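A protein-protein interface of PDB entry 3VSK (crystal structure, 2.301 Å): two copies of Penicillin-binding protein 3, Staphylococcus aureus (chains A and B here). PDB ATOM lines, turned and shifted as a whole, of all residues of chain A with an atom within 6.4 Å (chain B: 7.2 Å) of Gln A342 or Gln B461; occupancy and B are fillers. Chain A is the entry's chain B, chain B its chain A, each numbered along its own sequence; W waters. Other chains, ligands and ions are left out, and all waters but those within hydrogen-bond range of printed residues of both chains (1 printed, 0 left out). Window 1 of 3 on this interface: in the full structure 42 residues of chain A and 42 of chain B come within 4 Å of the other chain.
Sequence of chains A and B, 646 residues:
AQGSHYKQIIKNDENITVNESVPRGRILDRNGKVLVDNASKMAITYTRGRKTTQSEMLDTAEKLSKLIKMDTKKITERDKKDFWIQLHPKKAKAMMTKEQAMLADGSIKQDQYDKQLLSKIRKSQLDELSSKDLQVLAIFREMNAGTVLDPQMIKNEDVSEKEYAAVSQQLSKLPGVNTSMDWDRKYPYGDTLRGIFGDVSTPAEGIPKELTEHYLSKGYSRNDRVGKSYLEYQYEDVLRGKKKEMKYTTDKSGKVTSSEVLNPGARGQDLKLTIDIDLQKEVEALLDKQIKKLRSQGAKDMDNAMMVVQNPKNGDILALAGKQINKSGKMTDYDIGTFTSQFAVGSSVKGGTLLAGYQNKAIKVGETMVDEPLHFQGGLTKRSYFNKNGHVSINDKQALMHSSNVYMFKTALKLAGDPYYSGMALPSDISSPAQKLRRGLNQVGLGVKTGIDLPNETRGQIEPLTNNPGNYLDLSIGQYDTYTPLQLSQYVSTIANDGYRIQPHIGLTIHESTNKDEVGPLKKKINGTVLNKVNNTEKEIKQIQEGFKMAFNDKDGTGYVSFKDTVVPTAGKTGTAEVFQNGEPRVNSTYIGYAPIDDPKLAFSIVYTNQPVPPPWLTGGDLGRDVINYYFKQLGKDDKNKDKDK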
ATOM      1  N   ASN A 304       2.480   6.986  19.018  1.00  0.00           N
ATOM      2  CA  ASN A 304       2.982   8.343  18.963  1.00  0.00           C
ATOM      3  C   ASN A 304       3.269   8.733  17.530  1.00  0.00           C
ATOM      4  O   ASN A 304       3.892   7.981  16.782  1.00  0.00           O
ATOM      5  CB  ASN A 304       4.279   8.475  19.777  1.00  0.00           C
ATOM      6  CG  ASN A 304       4.039   8.650  21.279  1.00  0.00           C
ATOM      7  OD1 ASN A 304       3.153   9.404  21.703  1.00  0.00           O
ATOM      8  ND2 ASN A 304       4.854   7.970  22.091  1.00  0.00           N
ATOM      9  N   TYR A 334      -0.925  16.181  21.589  1.00  0.00           N
ATOM     10  CA  TYR A 334       0.385  15.958  22.192  1.00  0.00           C
ATOM     11  C   TYR A 334       1.467  16.717  21.435  1.00  0.00           C
ATOM     12  O   TYR A 334       2.560  16.197  21.253  1.00  0.00           O
ATOM     13  CB  TYR A 334       0.704  14.448  22.218  1.00  0.00           C
ATOM     14  CG  TYR A 334       1.852  14.063  23.127  1.00  0.00           C
ATOM     15  CD1 TYR A 334       2.305  14.932  24.123  1.00  0.00           C
ATOM     16  CD2 TYR A 334       2.490  12.836  22.984  1.00  0.00           C
ATOM     17  CE1 TYR A 334       3.368  14.583  24.963  1.00  0.00           C
ATOM     18  CE2 TYR A 334       3.546  12.476  23.793  1.00  0.00           C
ATOM     19  CZ  TYR A 334       3.987  13.350  24.786  1.00  0.00           C
ATOM     20  OH  TYR A 334       5.033  12.978  25.593  1.00  0.00           O
ATOM     21  N   GLY A 337       4.916  17.175  22.760  1.00  0.00           N
ATOM     22  CA  GLY A 337       5.763  16.012  22.652  1.00  0.00           C
ATOM     23  C   GLY A 337       6.997  16.268  21.824  1.00  0.00           C
ATOM     24  O   GLY A 337       8.038  15.646  22.044  1.00  0.00           O
ATOM     25  N   THR A 340       9.596  17.701  24.272  1.00  0.00           N
ATOM     26  CA  THR A 340       9.645  17.213  25.665  1.00  0.00           C
ATOM     27  C   THR A 340       9.830  15.705  25.772  1.00  0.00           C
ATOM     28  O   THR A 340      10.235  15.198  26.818  1.00  0.00           O
ATOM     29  CB  THR A 340       8.374  17.560  26.442  1.00  0.00           C
ATOM     30  OG1 THR A 340       7.275  16.844  25.861  1.00  0.00           O
ATOM     31  CG2 THR A 340       8.101  19.096  26.421  1.00  0.00           C
ATOM     32  N   SER A 341       9.515  14.997  24.689  1.00  0.00           N
ATOM     33  CA  SER A 341       9.621  13.544  24.645  1.00  0.00           C
ATOM     34  C   SER A 341      10.844  13.088  23.853  1.00  0.00           C
ATOM     35  O   SER A 341      11.164  13.641  22.790  1.00  0.00           O
ATOM     36  CB  SER A 341       8.368  12.934  24.014  1.00  0.00           C
ATOM     37  OG  SER A 341       7.217  13.246  24.769  1.00  0.00           O
ATOM     38  N   GLN A 342      11.510  12.055  24.356  1.00  0.00           N
ATOM     39  CA  GLN A 342      12.684  11.518  23.678  1.00  0.00           C
ATOM     40  C   GLN A 342      12.357  10.181  23.015  1.00  0.00           C
ATOM     41  O   GLN A 342      11.705   9.322  23.604  1.00  0.00           O
ATOM     42  CB  GLN A 342      13.834  11.385  24.678  1.00  0.00           C
ATOM     43  CG  GLN A 342      13.357  11.271  26.127  1.00  0.00           C
ATOM     44  CD  GLN A 342      12.618   9.966  26.408  1.00  0.00           C
ATOM     45  OE1 GLN A 342      11.382   9.945  26.540  1.00  0.00           O
ATOM     46  NE2 GLN A 342      13.376   8.868  26.513  1.00  0.00           N
ATOM     47  N   PHE A 343      12.813   9.997  21.785  1.00  0.00           N
ATOM     48  CA  PHE A 343      12.448   8.788  21.064  1.00  0.00           C
ATOM     49  C   PHE A 343      13.621   8.186  20.316  1.00  0.00           C
ATOM     50  O   PHE A 343      14.394   8.907  19.678  1.00  0.00           O
ATOM     51  CB  PHE A 343      11.311   9.090  20.090  1.00  0.00           C
ATOM     52  CG  PHE A 343      10.020   9.456  20.765  1.00  0.00           C
ATOM     53  CD1 PHE A 343       9.492   8.644  21.762  1.00  0.00           C
ATOM     54  CD2 PHE A 343       9.334  10.609  20.411  1.00  0.00           C
ATOM     55  CE1 PHE A 343       8.298   8.971  22.397  1.00  0.00           C
ATOM     56  CE2 PHE A 343       8.136  10.945  21.039  1.00  0.00           C
ATOM     57  CZ  PHE A 343       7.615  10.120  22.038  1.00  0.00           C
ATOM     58  N   ALA A 344      13.753   6.862  20.385  1.00  0.00           N
ATOM     59  CA  ALA A 344      14.776   6.167  19.607  1.00  0.00           C
ATOM     60  C   ALA A 344      14.489   6.358  18.114  1.00  0.00           C
ATOM     61  O   ALA A 344      13.431   5.963  17.608  1.00  0.00           O
ATOM     62  CB  ALA A 344      14.838   4.701  19.988  1.00  0.00           C
ATOM     63  N   THR A 458      13.770  18.714  26.574  1.00  0.00           N
ATOM     64  CA  THR A 458      14.696  17.657  26.991  1.00  0.00           C
ATOM     65  C   THR A 458      15.734  17.438  25.926  1.00  0.00           C
ATOM     66  O   THR A 458      15.476  17.610  24.729  1.00  0.00           O
ATOM     67  CB  THR A 458      13.999  16.289  27.219  1.00  0.00           C
ATOM     68  OG1 THR A 458      13.419  15.842  25.988  1.00  0.00           O
ATOM     69  CG2 THR A 458      12.921  16.405  28.262  1.00  0.00           C
ATOM     70  N   ARG A 459      16.900  16.996  26.359  1.00  0.00           N
ATOM     71  CA  ARG A 459      18.008  16.882  25.439  1.00  0.00           C
ATOM     72  C   ARG A 459      18.180  15.451  25.009  1.00  0.00           C
ATOM     73  O   ARG A 459      18.994  15.169  24.134  1.00  0.00           O
ATOM     74  CB  ARG A 459      19.300  17.368  26.091  1.00  0.00           C
ATOM     75  CG  ARG A 459      19.907  16.347  26.977  1.00  0.00           C
ATOM     76  CD  ARG A 459      21.181  16.815  27.571  1.00  0.00           C
ATOM     77  NE  ARG A 459      21.579  15.867  28.597  1.00  0.00           N
ATOM     78  CZ  ARG A 459      22.833  15.625  28.951  1.00  0.00           C
ATOM     79  NH1 ARG A 459      23.819  16.273  28.343  1.00  0.00           N
ATOM     80  NH2 ARG A 459      23.090  14.724  29.902  1.00  0.00           N
ATOM     81  N   GLY A 460      17.424  14.548  25.630  1.00  0.00           N
ATOM     82  CA  GLY A 460      17.562  13.125  25.345  1.00  0.00           C
ATOM     83  C   GLY A 460      18.178  12.313  26.476  1.00  0.00           C
ATOM     84  O   GLY A 460      18.909  12.852  27.310  1.00  0.00           O
ATOM     85  N   GLN A 461      17.875  11.015  26.513  1.00  0.00           N
ATOM     86  CA  GLN A 461      18.479  10.119  27.495  1.00  0.00           C
ATOM     87  C   GLN A 461      19.910   9.800  27.052  1.00  0.00           C
ATOM     88  O   GLN A 461      20.119   9.277  25.958  1.00  0.00           O
ATOM     89  CB  GLN A 461      17.637   8.842  27.662  1.00  0.00           C
ATOM     90  CG  GLN A 461      18.271   7.759  28.565  1.00  0.00           C
ATOM     91  CD  GLN A 461      17.504   7.503  29.873  1.00  0.00           C
ATOM     92  OE1 GLN A 461      17.191   8.443  30.631  1.00  0.00           O
ATOM     93  NE2 GLN A 461      17.216   6.216  30.149  1.00  0.00           N
ATOM     94  N   THR A 482      18.443   8.742  22.627  1.00  0.00           N
ATOM     95  CA  THR A 482      17.154   9.200  22.155  1.00  0.00           C
ATOM     96  C   THR A 482      17.212  10.686  21.898  1.00  0.00           C
ATOM     97  O   THR A 482      17.885  11.433  22.615  1.00  0.00           O
ATOM     98  CB  THR A 482      16.069   8.943  23.204  1.00  0.00           C
ATOM     99  OG1 THR A 482      16.583   9.262  24.503  1.00  0.00           O
ATOM    100  CG2 THR A 482      15.643   7.489  23.193  1.00  0.00           C
ATOM    101  N   TYR A 483      16.501  11.114  20.868  1.00  0.00           N
ATOM    102  CA  TYR A 483      16.369  12.524  20.589  1.00  0.00           C
ATOM    103  C   TYR A 483      14.904  12.909  20.544  1.00  0.00           C
ATOM    104  O   TYR A 483      14.012  12.087  20.746  1.00  0.00           O
ATOM    105  CB  TYR A 483      17.035  12.854  19.258  1.00  0.00           C
ATOM    106  CG  TYR A 483      18.475  12.452  19.205  1.00  0.00           C
ATOM    107  CD1 TYR A 483      19.386  12.891  20.172  1.00  0.00           C
ATOM    108  CD2 TYR A 483      18.929  11.628  18.197  1.00  0.00           C
ATOM    109  CE1 TYR A 483      20.716  12.511  20.114  1.00  0.00           C
ATOM    110  CE2 TYR A 483      20.248  11.239  18.135  1.00  0.00           C
ATOM    111  CZ  TYR A 483      21.136  11.686  19.092  1.00  0.00           C
ATOM    112  OH  TYR A 483      22.447  11.300  19.013  1.00  0.00           O
ATOM    113  N   THR A 484      14.661  14.180  20.277  1.00  0.00           N
ATOM    114  CA  THR A 484      13.292  14.662  20.149  1.00  0.00           C
ATOM    115  C   THR A 484      13.050  15.028  18.680  1.00  0.00           C
ATOM    116  O   THR A 484      13.998  15.191  17.910  1.00  0.00           O
ATOM    117  CB  THR A 484      13.078  15.864  21.077  1.00  0.00           C
ATOM    118  OG1 THR A 484      13.810  16.978  20.563  1.00  0.00           O
ATOM    119  CG2 THR A 484      13.600  15.557  22.450  1.00  0.00           C
ATOM    120  N   PRO A 485      11.784  15.137  18.277  1.00  0.00           N
ATOM    121  CA  PRO A 485      11.493  15.639  16.931  1.00  0.00           C
ATOM    122  C   PRO A 485      12.121  17.011  16.667  1.00  0.00           C
ATOM    123  O   PRO A 485      12.620  17.259  15.554  1.00  0.00           O
ATOM    124  CB  PRO A 485       9.967  15.742  16.938  1.00  0.00           C
ATOM    125  CG  PRO A 485       9.551  14.591  17.802  1.00  0.00           C
ATOM    126  CD  PRO A 485      10.601  14.507  18.894  1.00  0.00           C
ATOM    127  N   GLN B 342      15.978   9.049  34.167  1.00  0.00           N
ATOM    128  CA  GLN B 342      14.567   9.000  34.507  1.00  0.00           C
ATOM    129  C   GLN B 342      14.120   7.521  34.563  1.00  0.00           C
ATOM    130  O   GLN B 342      14.327   6.741  33.630  1.00  0.00           O
ATOM    131  CB  GLN B 342      13.818   9.913  33.490  1.00  0.00           C
ATOM    132  CG  GLN B 342      12.599   9.392  32.758  1.00  0.00           C
ATOM    133  CD  GLN B 342      12.878   8.358  31.676  1.00  0.00           C
ATOM    134  OE1 GLN B 342      14.028   8.153  31.285  1.00  0.00           O
ATOM    135  NE2 GLN B 342      11.817   7.696  31.186  1.00  0.00           N
ATOM    136  N   PHE B 343      13.551   7.122  35.691  1.00  0.00           N
ATOM    137  CA  PHE B 343      13.222   5.734  35.899  1.00  0.00           C
ATOM    138  C   PHE B 343      11.795   5.464  36.416  1.00  0.00           C
ATOM    139  O   PHE B 343      11.231   6.222  37.230  1.00  0.00           O
ATOM    140  CB  PHE B 343      14.251   5.125  36.850  1.00  0.00           C
ATOM    141  CG  PHE B 343      15.666   5.197  36.334  1.00  0.00           C
ATOM    142  CD1 PHE B 343      16.006   4.601  35.123  1.00  0.00           C
ATOM    143  CD2 PHE B 343      16.656   5.852  37.057  1.00  0.00           C
ATOM    144  CE1 PHE B 343      17.308   4.654  34.650  1.00  0.00           C
ATOM    145  CE2 PHE B 343      17.961   5.912  36.587  1.00  0.00           C
ATOM    146  CZ  PHE B 343      18.287   5.304  35.378  1.00  0.00           C
ATOM    147  N   ARG B 438      -1.329  14.610  39.488  1.00  0.00           N
ATOM    148  CA  ARG B 438      -0.023  15.175  39.109  1.00  0.00           C
ATOM    149  C   ARG B 438       0.353  16.444  39.884  1.00  0.00           C
ATOM    150  O   ARG B 438       1.502  16.615  40.278  1.00  0.00           O
ATOM    151  CB  ARG B 438       0.013  15.467  37.601  1.00  0.00           C
ATOM    152  CG  ARG B 438       0.172  14.210  36.748  1.00  0.00           C
ATOM    153  CD  ARG B 438       0.376  14.507  35.284  1.00  0.00           C
ATOM    154  NE  ARG B 438       1.044  13.385  34.642  1.00  0.00           N
ATOM    155  CZ  ARG B 438       0.713  12.904  33.451  1.00  0.00           C
ATOM    156  NH1 ARG B 438      -0.266  13.460  32.761  1.00  0.00           N
ATOM    157  NH2 ARG B 438       1.375  11.881  32.948  1.00  0.00           N
ATOM    158  N   THR B 458      16.490  16.540  34.451  1.00  0.00           N
ATOM    159  CA  THR B 458      15.194  16.264  33.801  1.00  0.00           C
ATOM    160  C   THR B 458      14.134  16.141  34.847  1.00  0.00           C
ATOM    161  O   THR B 458      14.428  15.905  36.023  1.00  0.00           O
ATOM    162  CB  THR B 458      15.141  14.934  33.009  1.00  0.00           C
ATOM    163  OG1 THR B 458      15.326  13.843  33.914  1.00  0.00           O
ATOM    164  CG2 THR B 458      16.208  14.891  31.935  1.00  0.00           C
ATOM    165  N   ARG B 459      12.896  16.247  34.396  1.00  0.00           N
ATOM    166  CA  ARG B 459      11.760  16.175  35.289  1.00  0.00           C
ATOM    167  C   ARG B 459      11.050  14.820  35.141  1.00  0.00           C
ATOM    168  O   ARG B 459      10.106  14.521  35.870  1.00  0.00           O
ATOM    169  CB  ARG B 459      10.794  17.313  34.983  1.00  0.00           C
ATOM    170  CG  ARG B 459       9.904  16.987  33.787  1.00  0.00           C
ATOM    171  CD  ARG B 459       9.098  18.185  33.304  1.00  0.00           C
ATOM    172  NE  ARG B 459       8.364  17.821  32.094  1.00  0.00           N
ATOM    173  CZ  ARG B 459       7.259  18.418  31.685  1.00  0.00           C
ATOM    174  NH1 ARG B 459       6.766  19.414  32.391  1.00  0.00           N
ATOM    175  NH2 ARG B 459       6.658  18.017  30.574  1.00  0.00           N
ATOM    176  N   GLY B 460      11.497  14.006  34.186  1.00  0.00           N
ATOM    177  CA  GLY B 460      10.888  12.710  33.956  1.00  0.00           C
ATOM    178  C   GLY B 460       9.909  12.695  32.798  1.00  0.00           C
ATOM    179  O   GLY B 460       9.404  13.727  32.380  1.00  0.00           O
ATOM    180  N   GLN B 461       9.634  11.511  32.273  1.00  0.00           N
ATOM    181  CA  GLN B 461       8.757  11.396  31.110  1.00  0.00           C
ATOM    182  C   GLN B 461       7.294  11.579  31.521  1.00  0.00           C
ATOM    183  O   GLN B 461       6.789  10.871  32.409  1.00  0.00           O
ATOM    184  CB  GLN B 461       8.948  10.044  30.425  1.00  0.00           C
ATOM    185  CG  GLN B 461       8.019   9.817  29.237  1.00  0.00           C
ATOM    186  CD  GLN B 461       8.013   8.369  28.761  1.00  0.00           C
ATOM    187  OE1 GLN B 461       7.785   7.441  29.548  1.00  0.00           O
ATOM    188  NE2 GLN B 461       8.259   8.173  27.461  1.00  0.00           N
ATOM    189  N   ILE B 462       6.619  12.535  30.875  1.00  0.00           N
ATOM    190  CA  ILE B 462       5.273  12.933  31.278  1.00  0.00           C
ATOM    191  C   ILE B 462       4.296  12.974  30.105  1.00  0.00           C
ATOM    192  O   ILE B 462       4.129  13.986  29.436  1.00  0.00           O
ATOM    193  CB  ILE B 462       5.260  14.302  31.986  1.00  0.00           C
ATOM    194  CG1 ILE B 462       6.241  14.316  33.157  1.00  0.00           C
ATOM    195  CG2 ILE B 462       3.845  14.633  32.468  1.00  0.00           C
ATOM    196  CD1 ILE B 462       6.271  15.634  33.900  1.00  0.00           C
ATOM    197  N   GLU B 463       3.639  11.850  29.889  1.00  0.00           N
ATOM    198  CA  GLU B 463       2.794  11.658  28.723  1.00  0.00           C
ATOM    199  C   GLU B 463       1.309  11.916  28.995  1.00  0.00           C
ATOM    200  O   GLU B 463       0.833  11.739  30.133  1.00  0.00           O
ATOM    201  CB  GLU B 463       3.013  10.248  28.188  1.00  0.00           C
ATOM    202  CG  GLU B 463       4.192  10.146  27.261  1.00  0.00           C
ATOM    203  CD  GLU B 463       4.759   8.742  27.208  1.00  0.00           C
ATOM    204  OE1 GLU B 463       5.676   8.535  26.380  1.00  0.00           O
ATOM    205  OE2 GLU B 463       4.302   7.855  27.988  1.00  0.00           O
ATOM    206  N   TYR B 480       3.484   4.844  35.890  1.00  0.00           N
ATOM    207  CA  TYR B 480       3.378   5.570  34.637  1.00  0.00           C
ATOM    208  C   TYR B 480       4.551   6.544  34.518  1.00  0.00           C
ATOM    209  O   TYR B 480       5.594   6.197  33.975  1.00  0.00           O
ATOM    210  CB  TYR B 480       2.040   6.287  34.525  1.00  0.00           C
ATOM    211  CG  TYR B 480       1.653   6.620  33.102  1.00  0.00           C
ATOM    212  CD1 TYR B 480       1.723   5.668  32.102  1.00  0.00           C
ATOM    213  CD2 TYR B 480       1.177   7.877  32.766  1.00  0.00           C
ATOM    214  CE1 TYR B 480       1.349   5.962  30.800  1.00  0.00           C
ATOM    215  CE2 TYR B 480       0.807   8.180  31.471  1.00  0.00           C
ATOM    216  CZ  TYR B 480       0.888   7.218  30.496  1.00  0.00           C
ATOM    217  OH  TYR B 480       0.519   7.519  29.205  1.00  0.00           O
ATOM    218  N   ASP B 481       4.381   7.759  35.030  1.00  0.00           N
ATOM    219  CA  ASP B 481       5.403   8.798  34.907  1.00  0.00           C
ATOM    220  C   ASP B 481       6.707   8.338  35.544  1.00  0.00           C
ATOM    221  O   ASP B 481       6.710   7.870  36.676  1.00  0.00           O
ATOM    222  CB  ASP B 481       4.917  10.087  35.572  1.00  0.00           C
ATOM    223  CG  ASP B 481       3.731  10.704  34.855  1.00  0.00           C
ATOM    224  OD1 ASP B 481       3.067   9.996  34.087  1.00  0.00           O
ATOM    225  OD2 ASP B 481       3.446  11.915  35.028  1.00  0.00           O
ATOM    226  N   THR B 482       7.808   8.456  34.810  1.00  0.00           N
ATOM    227  CA  THR B 482       9.122   8.136  35.362  1.00  0.00           C
ATOM    228  C   THR B 482       9.684   9.320  36.151  1.00  0.00           C
ATOM    229  O   THR B 482       9.525  10.485  35.747  1.00  0.00           O
ATOM    230  CB  THR B 482      10.110   7.804  34.255  1.00  0.00           C
ATOM    231  OG1 THR B 482       9.924   8.755  33.210  1.00  0.00           O
ATOM    232  CG2 THR B 482       9.858   6.421  33.669  1.00  0.00           C
ATOM    233  N   TYR B 483      10.349   9.007  37.264  1.00  0.00           N
ATOM    234  CA  TYR B 483      10.975  10.008  38.103  1.00  0.00           C
ATOM    235  C   TYR B 483      12.459   9.799  38.228  1.00  0.00           C
ATOM    236  O   TYR B 483      13.013   8.801  37.765  1.00  0.00           O
ATOM    237  CB  TYR B 483      10.371  10.022  39.504  1.00  0.00           C
ATOM    238  CG  TYR B 483       8.898  10.254  39.492  1.00  0.00           C
ATOM    239  CD1 TYR B 483       8.356  11.482  39.097  1.00  0.00           C
ATOM    240  CD2 TYR B 483       8.045   9.247  39.864  1.00  0.00           C
ATOM    241  CE1 TYR B 483       6.982  11.679  39.080  1.00  0.00           C
ATOM    242  CE2 TYR B 483       6.700   9.426  39.860  1.00  0.00           C
ATOM    243  CZ  TYR B 483       6.162  10.630  39.475  1.00  0.00           C
ATOM    244  OH  TYR B 483       4.796  10.731  39.475  1.00  0.00           O
ATOM    245  N   GLN B 487      14.589  13.527  42.507  1.00  0.00           N
ATOM    246  CA  GLN B 487      13.167  13.780  42.770  1.00  0.00           C
ATOM    247  C   GLN B 487      12.685  12.968  43.976  1.00  0.00           C
ATOM    248  O   GLN B 487      12.057  13.510  44.895  1.00  0.00           O
ATOM    249  CB  GLN B 487      12.317  13.465  41.534  1.00  0.00           C
ATOM    250  CG  GLN B 487      12.499  14.425  40.381  1.00  0.00           C
ATOM    251  CD  GLN B 487      11.546  14.188  39.225  1.00  0.00           C
ATOM    252  OE1 GLN B 487      11.590  13.145  38.576  1.00  0.00           O
ATOM    253  NE2 GLN B 487      10.675  15.166  38.960  1.00  0.00           N
HETATM  254  O   HOH W   1       5.760   6.236  24.245  1.00  0.00           O
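OE1 of Gln A461 sits close to OE1 of Gln B342 (3.2 Å).
NE2 of Gln B342 lies close to OG1 of Thr B482 (3.0 Å). NH2 of Arg B438 sits at hydrogen-bond distance from O of Glu B463, at 2.9 Å. The side-chain carboxylate (OE1) of Glu B463 lies within hydrogen-bond range of the side-chain amide nitrogen (NE2) of Gln B461 (2.8 Å). The backbone NH (N) of Gln B461 is in hydrogen-bond range of the side-chain hydroxyl (OG1) of Thr B482, at 2.9 Å. The backbone NH (N) of Gln A461 is in hydrogen-bond range of the side-chain hydroxyl (OG1) of Thr A482 (3.0 Å).
CG of Glu B463 touches OH of Tyr A334 (3.4 Å). Gln A342 touches Gln B461.
Of chain A, only Gln A342 comes within 4 Å of Gln B461. Of the printed residues of chain A, Glu B463 touches Tyr A334 (3.4 Å). Printed residues of chain B within 4 Å of Tyr A334: Glu B463. The nearest residue of chain B that does not touch Gln A342 is Gln B342 (4.9 Å). The nearest residue of chain A that does not touch Gln B461 is Phe A343 (5.1 Å).
Of the 14 printed residues of chain B, 3 touch a printed residue of chain A. Of the 16 printed residues of chain A, 3 touch a printed residue of chain B. Hydrophobic or aromatic side chains of chain A that line the printed part of chain B: Tyr A334. Among the printed residues, 3 pairs touch across the chains.
Gln A342 touches Gln B461, and with the chains exchanged Gln A461 touches Gln B342. Of the 3 pairs that touch across the chains among the printed residues, 2 have their exchanged pair printed and touching as well.
Water W1 bridges the side-chain amide nitrogen (ND2) of Asn A304 and the side-chain carboxylate (OE1) of Glu B463.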
